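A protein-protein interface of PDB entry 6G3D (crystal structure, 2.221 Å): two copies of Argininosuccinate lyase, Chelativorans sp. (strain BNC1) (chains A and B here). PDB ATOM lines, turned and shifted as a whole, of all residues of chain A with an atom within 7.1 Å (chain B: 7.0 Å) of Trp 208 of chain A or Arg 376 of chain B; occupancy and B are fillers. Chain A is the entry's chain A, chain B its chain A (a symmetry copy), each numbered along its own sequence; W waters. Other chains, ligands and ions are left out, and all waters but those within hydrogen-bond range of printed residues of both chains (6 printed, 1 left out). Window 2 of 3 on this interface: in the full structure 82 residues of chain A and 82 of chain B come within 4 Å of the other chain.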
ATOM      1  N   LEU A  54     -13.017 -23.072  -3.554  1.00  0.00           N
ATOM      2  CA  LEU A  54     -12.995 -22.087  -4.630  1.00  0.00           C
ATOM      3  C   LEU A  54     -13.494 -20.730  -4.152  1.00  0.00           C
ATOM      4  O   LEU A  54     -13.024 -19.691  -4.629  1.00  0.00           O
ATOM      5  CB  LEU A  54     -13.843 -22.559  -5.815  1.00  0.00           C
ATOM      6  CG  LEU A  54     -13.438 -23.809  -6.602  1.00  0.00           C
ATOM      7  CD1 LEU A  54     -14.437 -24.087  -7.724  1.00  0.00           C
ATOM      8  CD2 LEU A  54     -12.033 -23.670  -7.156  1.00  0.00           C
ATOM      9  N   GLN A  57     -10.803 -18.983  -2.190  1.00  0.00           N
ATOM     10  CA  GLN A  57      -9.731 -18.546  -3.071  1.00  0.00           C
ATOM     11  C   GLN A  57     -10.129 -17.382  -3.967  1.00  0.00           C
ATOM     12  O   GLN A  57      -9.262 -16.828  -4.650  1.00  0.00           O
ATOM     13  CB  GLN A  57      -9.257 -19.718  -3.934  1.00  0.00           C
ATOM     14  CG  GLN A  57      -8.574 -20.828  -3.151  1.00  0.00           C
ATOM     15  CD  GLN A  57      -7.442 -20.318  -2.277  1.00  0.00           C
ATOM     16  OE1 GLN A  57      -7.641 -19.995  -1.103  1.00  0.00           O
ATOM     17  NE2 GLN A  57      -6.247 -20.236  -2.849  1.00  0.00           N
ATOM     18  N   GLY A  58     -11.401 -16.992  -3.979  1.00  0.00           N
ATOM     19  CA  GLY A  58     -11.842 -15.939  -4.868  1.00  0.00           C
ATOM     20  C   GLY A  58     -12.108 -16.374  -6.289  1.00  0.00           C
ATOM     21  O   GLY A  58     -12.309 -15.516  -7.156  1.00  0.00           O
ATOM     22  N   ILE A  59     -12.101 -17.679  -6.561  1.00  0.00           N
ATOM     23  CA  ILE A  59     -12.455 -18.166  -7.888  1.00  0.00           C
ATOM     24  C   ILE A  59     -13.964 -18.098  -8.092  1.00  0.00           C
ATOM     25  O   ILE A  59     -14.446 -17.813  -9.195  1.00  0.00           O
ATOM     26  CB  ILE A  59     -11.907 -19.592  -8.084  1.00  0.00           C
ATOM     27  CG1 ILE A  59     -10.376 -19.575  -8.031  1.00  0.00           C
ATOM     28  CG2 ILE A  59     -12.385 -20.184  -9.399  1.00  0.00           C
ATOM     29  CD1 ILE A  59      -9.753 -20.913  -7.687  1.00  0.00           C
ATOM     30  N   LYS A 105     -19.226 -24.010 -13.312  1.00  0.00           N
ATOM     31  CA  LYS A 105     -18.060 -23.475 -12.618  1.00  0.00           C
ATOM     32  C   LYS A 105     -17.598 -24.353 -11.462  1.00  0.00           C
ATOM     33  O   LYS A 105     -16.482 -24.160 -10.971  1.00  0.00           O
ATOM     34  CB  LYS A 105     -18.344 -22.063 -12.103  1.00  0.00           C
ATOM     35  CG  LYS A 105     -18.266 -20.982 -13.165  1.00  0.00           C
ATOM     36  CD  LYS A 105     -18.138 -19.607 -12.530  1.00  0.00           C
ATOM     37  CE  LYS A 105     -17.700 -18.568 -13.548  1.00  0.00           C
ATOM     38  NZ  LYS A 105     -17.549 -17.223 -12.927  1.00  0.00           N
ATOM     39  N   HIS A 107     -16.596 -27.243 -11.604  1.00  0.00           N
ATOM     40  CA  HIS A 107     -15.556 -28.132 -12.100  1.00  0.00           C
ATOM     41  C   HIS A 107     -14.255 -27.399 -12.397  1.00  0.00           C
ATOM     42  O   HIS A 107     -13.343 -27.993 -12.981  1.00  0.00           O
ATOM     43  CB  HIS A 107     -16.041 -28.861 -13.353  1.00  0.00           C
ATOM     44  CG  HIS A 107     -15.489 -30.244 -13.496  1.00  0.00           C
ATOM     45  ND1 HIS A 107     -15.436 -31.132 -12.443  1.00  0.00           N
ATOM     46  CD2 HIS A 107     -14.984 -30.899 -14.568  1.00  0.00           C
ATOM     47  CE1 HIS A 107     -14.912 -32.271 -12.859  1.00  0.00           C
ATOM     48  NE2 HIS A 107     -14.628 -32.156 -14.145  1.00  0.00           N
ATOM     49  N   ILE A 108     -14.150 -26.125 -12.013  1.00  0.00           N
ATOM     50  CA  ILE A 108     -12.926 -25.367 -12.244  1.00  0.00           C
ATOM     51  C   ILE A 108     -11.774 -25.998 -11.474  1.00  0.00           C
ATOM     52  O   ILE A 108     -11.897 -26.312 -10.283  1.00  0.00           O
ATOM     53  CB  ILE A 108     -13.126 -23.897 -11.844  1.00  0.00           C
ATOM     54  CG1 ILE A 108     -14.028 -23.179 -12.851  1.00  0.00           C
ATOM     55  CG2 ILE A 108     -11.796 -23.186 -11.721  1.00  0.00           C
ATOM     56  CD1 ILE A 108     -14.608 -21.880 -12.332  1.00  0.00           C
ATOM     57  N   GLY A 109     -10.645 -26.183 -12.156  1.00  0.00           N
ATOM     58  CA  GLY A 109      -9.476 -26.778 -11.540  1.00  0.00           C
ATOM     59  C   GLY A 109      -9.639 -28.219 -11.123  1.00  0.00           C
ATOM     60  O   GLY A 109      -8.847 -28.710 -10.312  1.00  0.00           O
ATOM     61  N   ARG A 110     -10.637 -28.918 -11.658  1.00  0.00           N
ATOM     62  CA  ARG A 110     -10.955 -30.269 -11.231  1.00  0.00           C
ATOM     63  C   ARG A 110     -11.186 -31.142 -12.456  1.00  0.00           C
ATOM     64  O   ARG A 110     -11.485 -30.655 -13.550  1.00  0.00           O
ATOM     65  CB  ARG A 110     -12.191 -30.283 -10.316  1.00  0.00           C
ATOM     66  CG  ARG A 110     -12.384 -31.566  -9.519  1.00  0.00           C
ATOM     67  CD  ARG A 110     -13.592 -31.466  -8.601  1.00  0.00           C
ATOM     68  NE  ARG A 110     -14.824 -31.188  -9.332  1.00  0.00           N
ATOM     69  CZ  ARG A 110     -16.027 -31.132  -8.771  1.00  0.00           C
ATOM     70  NH1 ARG A 110     -16.157 -31.330  -7.467  1.00  0.00           N
ATOM     71  NH2 ARG A 110     -17.098 -30.872  -9.509  1.00  0.00           N
ATOM     72  N   GLY A 205      -2.207 -31.187 -12.245  1.00  0.00           N
ATOM     73  CA  GLY A 205      -2.536 -29.970 -11.529  1.00  0.00           C
ATOM     74  C   GLY A 205      -3.308 -28.997 -12.402  1.00  0.00           C
ATOM     75  O   GLY A 205      -4.006 -29.380 -13.347  1.00  0.00           O
ATOM     76  N   THR A 206      -3.172 -27.712 -12.083  1.00  0.00           N
ATOM     77  CA  THR A 206      -3.922 -26.679 -12.780  1.00  0.00           C
ATOM     78  C   THR A 206      -3.265 -25.332 -12.536  1.00  0.00           C
ATOM     79  O   THR A 206      -2.556 -25.133 -11.547  1.00  0.00           O
ATOM     80  CB  THR A 206      -5.387 -26.645 -12.327  1.00  0.00           C
ATOM     81  OG1 THR A 206      -6.061 -25.551 -12.963  1.00  0.00           O
ATOM     82  CG2 THR A 206      -5.470 -26.473 -10.819  1.00  0.00           C
ATOM     83  N   GLY A 207      -3.512 -24.404 -13.462  1.00  0.00           N
ATOM     84  CA  GLY A 207      -3.115 -23.025 -13.272  1.00  0.00           C
ATOM     85  C   GLY A 207      -4.020 -22.230 -12.362  1.00  0.00           C
ATOM     86  O   GLY A 207      -3.641 -21.137 -11.931  1.00  0.00           O
ATOM     87  N   TRP A 208      -5.207 -22.749 -12.072  1.00  0.00           N
ATOM     88  CA  TRP A 208      -6.089 -22.103 -11.116  1.00  0.00           C
ATOM     89  C   TRP A 208      -5.466 -22.157  -9.722  1.00  0.00           C
ATOM     90  O   TRP A 208      -4.888 -23.181  -9.339  1.00  0.00           O
ATOM     91  CB  TRP A 208      -7.459 -22.781 -11.115  1.00  0.00           C
ATOM     92  CG  TRP A 208      -8.273 -22.505 -12.347  1.00  0.00           C
ATOM     93  CD1 TRP A 208      -8.435 -23.325 -13.429  1.00  0.00           C
ATOM     94  CD2 TRP A 208      -9.052 -21.331 -12.615  1.00  0.00           C
ATOM     95  NE1 TRP A 208      -9.260 -22.730 -14.354  1.00  0.00           N
ATOM     96  CE2 TRP A 208      -9.653 -21.507 -13.879  1.00  0.00           C
ATOM     97  CE3 TRP A 208      -9.298 -20.149 -11.911  1.00  0.00           C
ATOM     98  CZ2 TRP A 208     -10.483 -20.542 -14.451  1.00  0.00           C
ATOM     99  CZ3 TRP A 208     -10.122 -19.195 -12.481  1.00  0.00           C
ATOM    100  CH2 TRP A 208     -10.706 -19.398 -13.737  1.00  0.00           C
ATOM    101  N   PRO A 209      -5.561 -21.067  -8.932  1.00  0.00           N
ATOM    102  CA  PRO A 209      -4.875 -21.000  -7.624  1.00  0.00           C
ATOM    103  C   PRO A 209      -5.645 -21.709  -6.518  1.00  0.00           C
ATOM    104  O   PRO A 209      -6.259 -21.101  -5.633  1.00  0.00           O
ATOM    105  CB  PRO A 209      -4.766 -19.489  -7.398  1.00  0.00           C
ATOM    106  CG  PRO A 209      -6.020 -18.953  -8.023  1.00  0.00           C
ATOM    107  CD  PRO A 209      -6.312 -19.834  -9.221  1.00  0.00           C
ATOM    108  N   LEU A 210      -5.617 -23.039  -6.557  1.00  0.00           N
ATOM    109  CA  LEU A 210      -6.315 -23.830  -5.559  1.00  0.00           C
ATOM    110  C   LEU A 210      -5.565 -23.807  -4.231  1.00  0.00           C
ATOM    111  O   LEU A 210      -4.372 -23.499  -4.163  1.00  0.00           O
ATOM    112  CB  LEU A 210      -6.486 -25.275  -6.032  1.00  0.00           C
ATOM    113  CG  LEU A 210      -7.070 -25.521  -7.424  1.00  0.00           C
ATOM    114  CD1 LEU A 210      -7.205 -27.017  -7.684  1.00  0.00           C
ATOM    115  CD2 LEU A 210      -8.408 -24.815  -7.597  1.00  0.00           C
ATOM    116  N   ASN A 211      -6.293 -24.120  -3.161  1.00  0.00           N
ATOM    117  CA  ASN A 211      -5.712 -24.384  -1.846  1.00  0.00           C
ATOM    118  C   ASN A 211      -6.037 -25.838  -1.522  1.00  0.00           C
ATOM    119  O   ASN A 211      -7.112 -26.139  -0.992  1.00  0.00           O
ATOM    120  CB  ASN A 211      -6.248 -23.427  -0.782  1.00  0.00           C
ATOM    121  CG  ASN A 211      -5.579 -23.622   0.572  1.00  0.00           C
ATOM    122  OD1 ASN A 211      -4.645 -24.412   0.707  1.00  0.00           O
ATOM    123  ND2 ASN A 211      -6.052 -22.894   1.578  1.00  0.00           N
ATOM    124  N   THR B 368      -6.223 -27.593 -22.546  1.00  0.00           N
ATOM    125  CA  THR B 368      -6.811 -27.258 -21.252  1.00  0.00           C
ATOM    126  C   THR B 368      -6.535 -25.805 -20.888  1.00  0.00           C
ATOM    127  O   THR B 368      -7.431 -25.088 -20.426  1.00  0.00           O
ATOM    128  CB  THR B 368      -6.267 -28.189 -20.169  1.00  0.00           C
ATOM    129  OG1 THR B 368      -6.684 -29.531 -20.438  1.00  0.00           O
ATOM    130  CG2 THR B 368      -6.777 -27.767 -18.800  1.00  0.00           C
ATOM    131  N   THR B 371      -8.666 -23.529 -22.793  1.00  0.00           N
ATOM    132  CA  THR B 371     -10.009 -23.533 -22.224  1.00  0.00           C
ATOM    133  C   THR B 371     -10.058 -22.717 -20.939  1.00  0.00           C
ATOM    134  O   THR B 371     -10.961 -21.893 -20.749  1.00  0.00           O
ATOM    135  CB  THR B 371     -10.462 -24.971 -21.964  1.00  0.00           C
ATOM    136  OG1 THR B 371     -10.264 -25.756 -23.147  1.00  0.00           O
ATOM    137  CG2 THR B 371     -11.929 -25.011 -21.580  1.00  0.00           C
ATOM    138  N   ASP B 372      -9.090 -22.933 -20.045  1.00  0.00           N
ATOM    139  CA  ASP B 372      -9.044 -22.170 -18.803  1.00  0.00           C
ATOM    140  C   ASP B 372      -8.875 -20.683 -19.070  1.00  0.00           C
ATOM    141  O   ASP B 372      -9.381 -19.855 -18.306  1.00  0.00           O
ATOM    142  CB  ASP B 372      -7.908 -22.673 -17.913  1.00  0.00           C
ATOM    143  CG  ASP B 372      -8.236 -23.983 -17.234  1.00  0.00           C
ATOM    144  OD1 ASP B 372      -9.435 -24.318 -17.134  1.00  0.00           O
ATOM    145  OD2 ASP B 372      -7.295 -24.675 -16.795  1.00  0.00           O
ATOM    146  N   MET B 373      -8.168 -20.325 -20.144  1.00  0.00           N
ATOM    147  CA  MET B 373      -7.962 -18.915 -20.456  1.00  0.00           C
ATOM    148  C   MET B 373      -9.261 -18.248 -20.883  1.00  0.00           C
ATOM    149  O   MET B 373      -9.534 -17.110 -20.490  1.00  0.00           O
ATOM    150  CB  MET B 373      -6.892 -18.769 -21.540  1.00  0.00           C
ATOM    151  CG  MET B 373      -6.461 -17.333 -21.819  1.00  0.00           C
ATOM    152  SD  MET B 373      -7.444 -16.540 -23.107  1.00  0.00           S
ATOM    153  CE  MET B 373      -6.831 -17.391 -24.559  1.00  0.00           C
ATOM    154  N   LEU B 374     -10.074 -18.936 -21.688  1.00  0.00           N
ATOM    155  CA  LEU B 374     -11.363 -18.375 -22.082  1.00  0.00           C
ATOM    156  C   LEU B 374     -12.243 -18.128 -20.861  1.00  0.00           C
ATOM    157  O   LEU B 374     -12.834 -17.052 -20.714  1.00  0.00           O
ATOM    158  CB  LEU B 374     -12.065 -19.305 -23.077  1.00  0.00           C
ATOM    159  CG  LEU B 374     -11.350 -19.603 -24.398  1.00  0.00           C
ATOM    160  CD1 LEU B 374     -12.242 -20.405 -25.340  1.00  0.00           C
ATOM    161  CD2 LEU B 374     -10.874 -18.323 -25.074  1.00  0.00           C
ATOM    162  N   VAL B 375     -12.325 -19.110 -19.962  1.00  0.00           N
ATOM    163  CA  VAL B 375     -13.151 -18.956 -18.765  1.00  0.00           C
ATOM    164  C   VAL B 375     -12.621 -17.826 -17.895  1.00  0.00           C
ATOM    165  O   VAL B 375     -13.379 -16.973 -17.419  1.00  0.00           O
ATOM    166  CB  VAL B 375     -13.216 -20.280 -17.982  1.00  0.00           C
ATOM    167  CG1 VAL B 375     -13.985 -20.095 -16.680  1.00  0.00           C
ATOM    168  CG2 VAL B 375     -13.843 -21.364 -18.825  1.00  0.00           C
ATOM    169  N   ARG B 376     -11.308 -17.795 -17.681  1.00  0.00           N
ATOM    170  CA  ARG B 376     -10.742 -16.867 -16.711  1.00  0.00           C
ATOM    171  C   ARG B 376     -10.593 -15.455 -17.273  1.00  0.00           C
ATOM    172  O   ARG B 376     -10.594 -14.486 -16.503  1.00  0.00           O
ATOM    173  CB  ARG B 376      -9.406 -17.423 -16.206  1.00  0.00           C
ATOM    174  CG  ARG B 376      -8.404 -16.428 -15.648  1.00  0.00           C
ATOM    175  CD  ARG B 376      -7.308 -17.155 -14.875  1.00  0.00           C
ATOM    176  NE  ARG B 376      -7.434 -16.989 -13.429  1.00  0.00           N
ATOM    177  CZ  ARG B 376      -6.575 -17.483 -12.542  1.00  0.00           C
ATOM    178  NH1 ARG B 376      -5.532 -18.194 -12.948  1.00  0.00           N
ATOM    179  NH2 ARG B 376      -6.762 -17.276 -11.245  1.00  0.00           N
ATOM    180  N   ARG B 377     -10.505 -15.307 -18.597  1.00  0.00           N
ATOM    181  CA  ARG B 377     -10.272 -14.001 -19.209  1.00  0.00           C
ATOM    182  C   ARG B 377     -11.526 -13.386 -19.824  1.00  0.00           C
ATOM    183  O   ARG B 377     -11.830 -12.221 -19.544  1.00  0.00           O
ATOM    184  CB  ARG B 377      -9.159 -14.100 -20.261  1.00  0.00           C
ATOM    185  CG  ARG B 377      -9.007 -12.876 -21.143  1.00  0.00           C
ATOM    186  CD  ARG B 377      -7.666 -12.192 -20.897  1.00  0.00           C
ATOM    187  NE  ARG B 377      -6.532 -13.093 -21.093  1.00  0.00           N
ATOM    188  CZ  ARG B 377      -5.377 -12.997 -20.439  1.00  0.00           C
ATOM    189  NH1 ARG B 377      -5.198 -12.038 -19.540  1.00  0.00           N
ATOM    190  NH2 ARG B 377      -4.401 -13.860 -20.682  1.00  0.00           N
ATOM    191  N   VAL B 378     -12.261 -14.123 -20.665  1.00  0.00           N
ATOM    192  CA  VAL B 378     -13.489 -13.586 -21.246  1.00  0.00           C
ATOM    193  C   VAL B 378     -14.724 -13.991 -20.463  1.00  0.00           C
ATOM    194  O   VAL B 378     -15.830 -13.548 -20.798  1.00  0.00           O
ATOM    195  CB  VAL B 378     -13.668 -13.983 -22.728  1.00  0.00           C
ATOM    196  CG1 VAL B 378     -12.404 -13.790 -23.480  1.00  0.00           C
ATOM    197  CG2 VAL B 378     -14.170 -15.406 -22.884  1.00  0.00           C
ATOM    198  N   GLY B 379     -14.576 -14.828 -19.441  1.00  0.00           N
ATOM    199  CA  GLY B 379     -15.679 -15.155 -18.562  1.00  0.00           C
ATOM    200  C   GLY B 379     -16.851 -15.840 -19.232  1.00  0.00           C
ATOM    201  O   GLY B 379     -17.991 -15.391 -19.089  1.00  0.00           O
ATOM    202  N   ILE B 380     -16.592 -16.912 -19.978  1.00  0.00           N
ATOM    203  CA  ILE B 380     -17.651 -17.781 -20.467  1.00  0.00           C
ATOM    204  C   ILE B 380     -17.749 -18.973 -19.525  1.00  0.00           C
ATOM    205  O   ILE B 380     -16.835 -19.265 -18.748  1.00  0.00           O
ATOM    206  CB  ILE B 380     -17.441 -18.243 -21.935  1.00  0.00           C
ATOM    207  CG1 ILE B 380     -15.986 -18.650 -22.190  1.00  0.00           C
ATOM    208  CG2 ILE B 380     -17.889 -17.156 -22.906  1.00  0.00           C
ATOM    209  CD1 ILE B 380     -15.727 -19.124 -23.612  1.00  0.00           C
ATOM    210  N   TYR B 382     -17.715 -22.740 -18.170  1.00  0.00           N
ATOM    211  CA  TYR B 382     -16.650 -23.698 -18.444  1.00  0.00           C
ATOM    212  C   TYR B 382     -17.065 -24.701 -19.512  1.00  0.00           C
ATOM    213  O   TYR B 382     -16.251 -25.083 -20.362  1.00  0.00           O
ATOM    214  CB  TYR B 382     -16.213 -24.434 -17.179  1.00  0.00           C
ATOM    215  CG  TYR B 382     -14.939 -25.197 -17.450  1.00  0.00           C
ATOM    216  CD1 TYR B 382     -14.970 -26.525 -17.858  1.00  0.00           C
ATOM    217  CD2 TYR B 382     -13.707 -24.568 -17.369  1.00  0.00           C
ATOM    218  CE1 TYR B 382     -13.804 -27.213 -18.142  1.00  0.00           C
ATOM    219  CE2 TYR B 382     -12.536 -25.245 -17.649  1.00  0.00           C
ATOM    220  CZ  TYR B 382     -12.590 -26.567 -18.035  1.00  0.00           C
ATOM    221  OH  TYR B 382     -11.421 -27.239 -18.312  1.00  0.00           O
ATOM    222  N   ARG B 442       2.682 -22.349 -15.299  1.00  0.00           N
ATOM    223  CA  ARG B 442       1.435 -21.968 -14.643  1.00  0.00           C
ATOM    224  C   ARG B 442       0.987 -22.986 -13.600  1.00  0.00           C
ATOM    225  O   ARG B 442       0.234 -22.627 -12.689  1.00  0.00           O
ATOM    226  CB  ARG B 442       0.328 -21.764 -15.681  1.00  0.00           C
ATOM    227  CG  ARG B 442       0.404 -20.433 -16.415  1.00  0.00           C
ATOM    228  CD  ARG B 442      -0.842 -20.186 -17.253  1.00  0.00           C
ATOM    229  NE  ARG B 442      -0.863 -20.999 -18.464  1.00  0.00           N
ATOM    230  CZ  ARG B 442      -0.300 -20.636 -19.612  1.00  0.00           C
ATOM    231  NH1 ARG B 442       0.332 -19.474 -19.702  1.00  0.00           N
ATOM    232  NH2 ARG B 442      -0.367 -21.436 -20.667  1.00  0.00           N
ATOM    233  N   ARG B 443       1.435 -24.237 -13.705  1.00  0.00           N
ATOM    234  CA  ARG B 443       1.070 -25.280 -12.746  1.00  0.00           C
ATOM    235  C   ARG B 443       2.141 -25.328 -11.660  1.00  0.00           C
ATOM    236  O   ARG B 443       3.003 -26.207 -11.625  1.00  0.00           O
ATOM    237  CB  ARG B 443       0.915 -26.621 -13.447  1.00  0.00           C
ATOM    238  CG  ARG B 443      -0.301 -26.696 -14.354  1.00  0.00           C
ATOM    239  CD  ARG B 443      -0.167 -27.806 -15.383  1.00  0.00           C
ATOM    240  NE  ARG B 443      -1.431 -28.072 -16.068  1.00  0.00           N
ATOM    241  CZ  ARG B 443      -1.947 -27.303 -17.023  1.00  0.00           C
ATOM    242  NH1 ARG B 443      -3.103 -27.630 -17.583  1.00  0.00           N
ATOM    243  NH2 ARG B 443      -1.305 -26.214 -17.426  1.00  0.00           N
ATOM    244  N   GLY B 445       1.457 -25.239  -8.206  1.00  0.00           N
ATOM    245  CA  GLY B 445       0.982 -25.688  -6.915  1.00  0.00           C
ATOM    246  C   GLY B 445       1.786 -26.863  -6.381  1.00  0.00           C
ATOM    247  O   GLY B 445       2.785 -27.302  -6.954  1.00  0.00           O
ATOM    248  N   MET B 448       2.893 -30.249  -8.538  1.00  0.00           N
ATOM    249  CA  MET B 448       2.667 -29.901  -9.928  1.00  0.00           C
ATOM    250  C   MET B 448       3.998 -29.733 -10.665  1.00  0.00           C
ATOM    251  O   MET B 448       5.054 -29.599 -10.038  1.00  0.00           O
ATOM    252  CB  MET B 448       1.822 -28.623 -10.006  1.00  0.00           C
ATOM    253  CG  MET B 448       0.434 -28.794  -9.394  1.00  0.00           C
ATOM    254  SD  MET B 448      -0.664 -27.381  -9.615  1.00  0.00           S
ATOM    255  CE  MET B 448      -1.976 -27.808  -8.470  1.00  0.00           C
HETATM  256  O   HOH W   1      -4.654 -24.379 -16.186  1.00  0.00           O
HETATM  257  O   HOH W   2      -0.840 -20.185 -12.144  1.00  0.00           O
HETATM  258  O   HOH W   3      -5.328 -28.513 -15.658  1.00  0.00           O
HETATM  259  O   HOH W   4     -10.219 -26.479 -14.897  1.00  0.00           O
HETATM  260  O   HOH W   5     -11.979 -28.565 -15.303  1.00  0.00           O
HETATM  261  O   HOH W   6      -7.209 -26.531 -15.134  1.00  0.00           O
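Hydrophobic or aromatic side chains of chain B within 4 Å of the printed part of chain A: Met 448. Of the 16 printed residues of chain A, 5 touch a printed residue of chain B. Printed residues of chain A that touch a printed residue of chain B: Gly 205, Thr 206, Gly 207, Trp 208 and Pro 209. Among the printed residues, 10 pairs touch across the chains.
Among the printed residues, merely in contact across the chains: Pro 209 of chain A with Arg 376 of chain B (3.3 Å), Trp 208 of chain A with Arg 376 of chain B (3.4 Å), Gly 207 of chain A with Arg 442 of chain B (3.4 Å), Gly 207 of chain A with Arg 376 of chain B (3.6 Å), Gly 205 of chain A with Met 448 of chain B (3.7 Å), Thr 206 of chain A with Arg 443 of chain B (3.7 Å), Thr 206 of chain A with Arg 442 of chain B (3.9 Å) and Gly 205 of chain A with Arg 443 of chain B (3.97 Å).
SD of Met 448 of chain B is in hydrogen-bond range of N of Thr 206 of chain A (3.5 Å). NE1 of Trp 208 of chain A is in hydrogen-bond range of OD1 of Asp 372 of chain B, at 3.2 Å.
No position is printed for both chains.
NE2 of Gln 57 of chain A is in hydrogen-bond range of O of Pro 209 of chain A (2.9 Å). N of Trp 208 of chain A sits at hydrogen-bond distance from OG1 of Thr 206 of chain A (3.1 Å). The backbone NH (N) of Gly 445 of chain B lies within hydrogen-bond range of the side-chain sulfur (SD) of Met 448 of chain B (3.3 Å).
Printed residues of chain B within 4 Å of Gly 205 of chain A: Arg 443 and Met 448. Gly 207 of chain A touches just these residues of chain B: Arg 376 and Arg 442. Trp 208 of chain A touches just these residues of chain B: Asp 372 and Arg 376. Printed residues of chain B within 4 Å of Pro 209 of chain A: Arg 376. Thr 371 of chain B touches none of the printed residues of chain A. Met 373 of chain B touches none of the printed residues of chain A. Of the printed residues of chain A, Arg 376 of chain B touches Gly 207 (3.6 Å), Trp 208 (3.4 Å) and Pro 209 (3.3 Å). Printed residues of chain A within 4 Å of Arg 442 of chain B: Thr 206 (3.9 Å) and Gly 207 (3.4 Å). Of the printed residues of chain A, Arg 443 of chain B touches Gly 205 (3.97 Å) and Thr 206 (3.7 Å). Of the printed residues of chain A, Met 448 of chain B touches Gly 205 (3.7 Å) and Thr 206 (3.5 Å). The nearest residue of chain B that does not touch Trp 208 of chain A is Val 375 of chain B (4.2 Å). The nearest printed residue of chain A that does not touch Met 448 of chain B is Leu 210 of chain A (5.3 Å).
Water W6 bridges OD2 of Asp 372 of chain B (2.5 Å) and OG1 of Thr 206 of chain A (2.6 Å). Water W2 lies within hydrogen-bond range of O of Arg 442 of chain B (2.7 Å) and O of Gly 207 of chain A (3.0 Å). Water W1 bridges the side-chain carboxylate (OD2) of Asp 372 of chain B and the backbone NH (N) of Gly 207 of chain A. Water W5 lies within hydrogen-bond range of the backbone carbonyl oxygen of His 107 of chain A (2.8 Å), the backbone carbonyl oxygen of Arg 110 of chain A (2.8 Å) and the side-chain hydroxyl of Tyr 382 of chain B (3.3 Å). Water W4 lies within hydrogen-bond range of the backbone NH (N) of Gly 109 of chain A (2.8 Å) and the side-chain carboxylate (OD1) of Asp 372 of chain B (3.2 Å). Water W3 lies within hydrogen-bond range of the backbone carbonyl oxygen (O) of Gly 205 of chain A and the guanidinium group (NH1) of Arg 443 of chain B.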
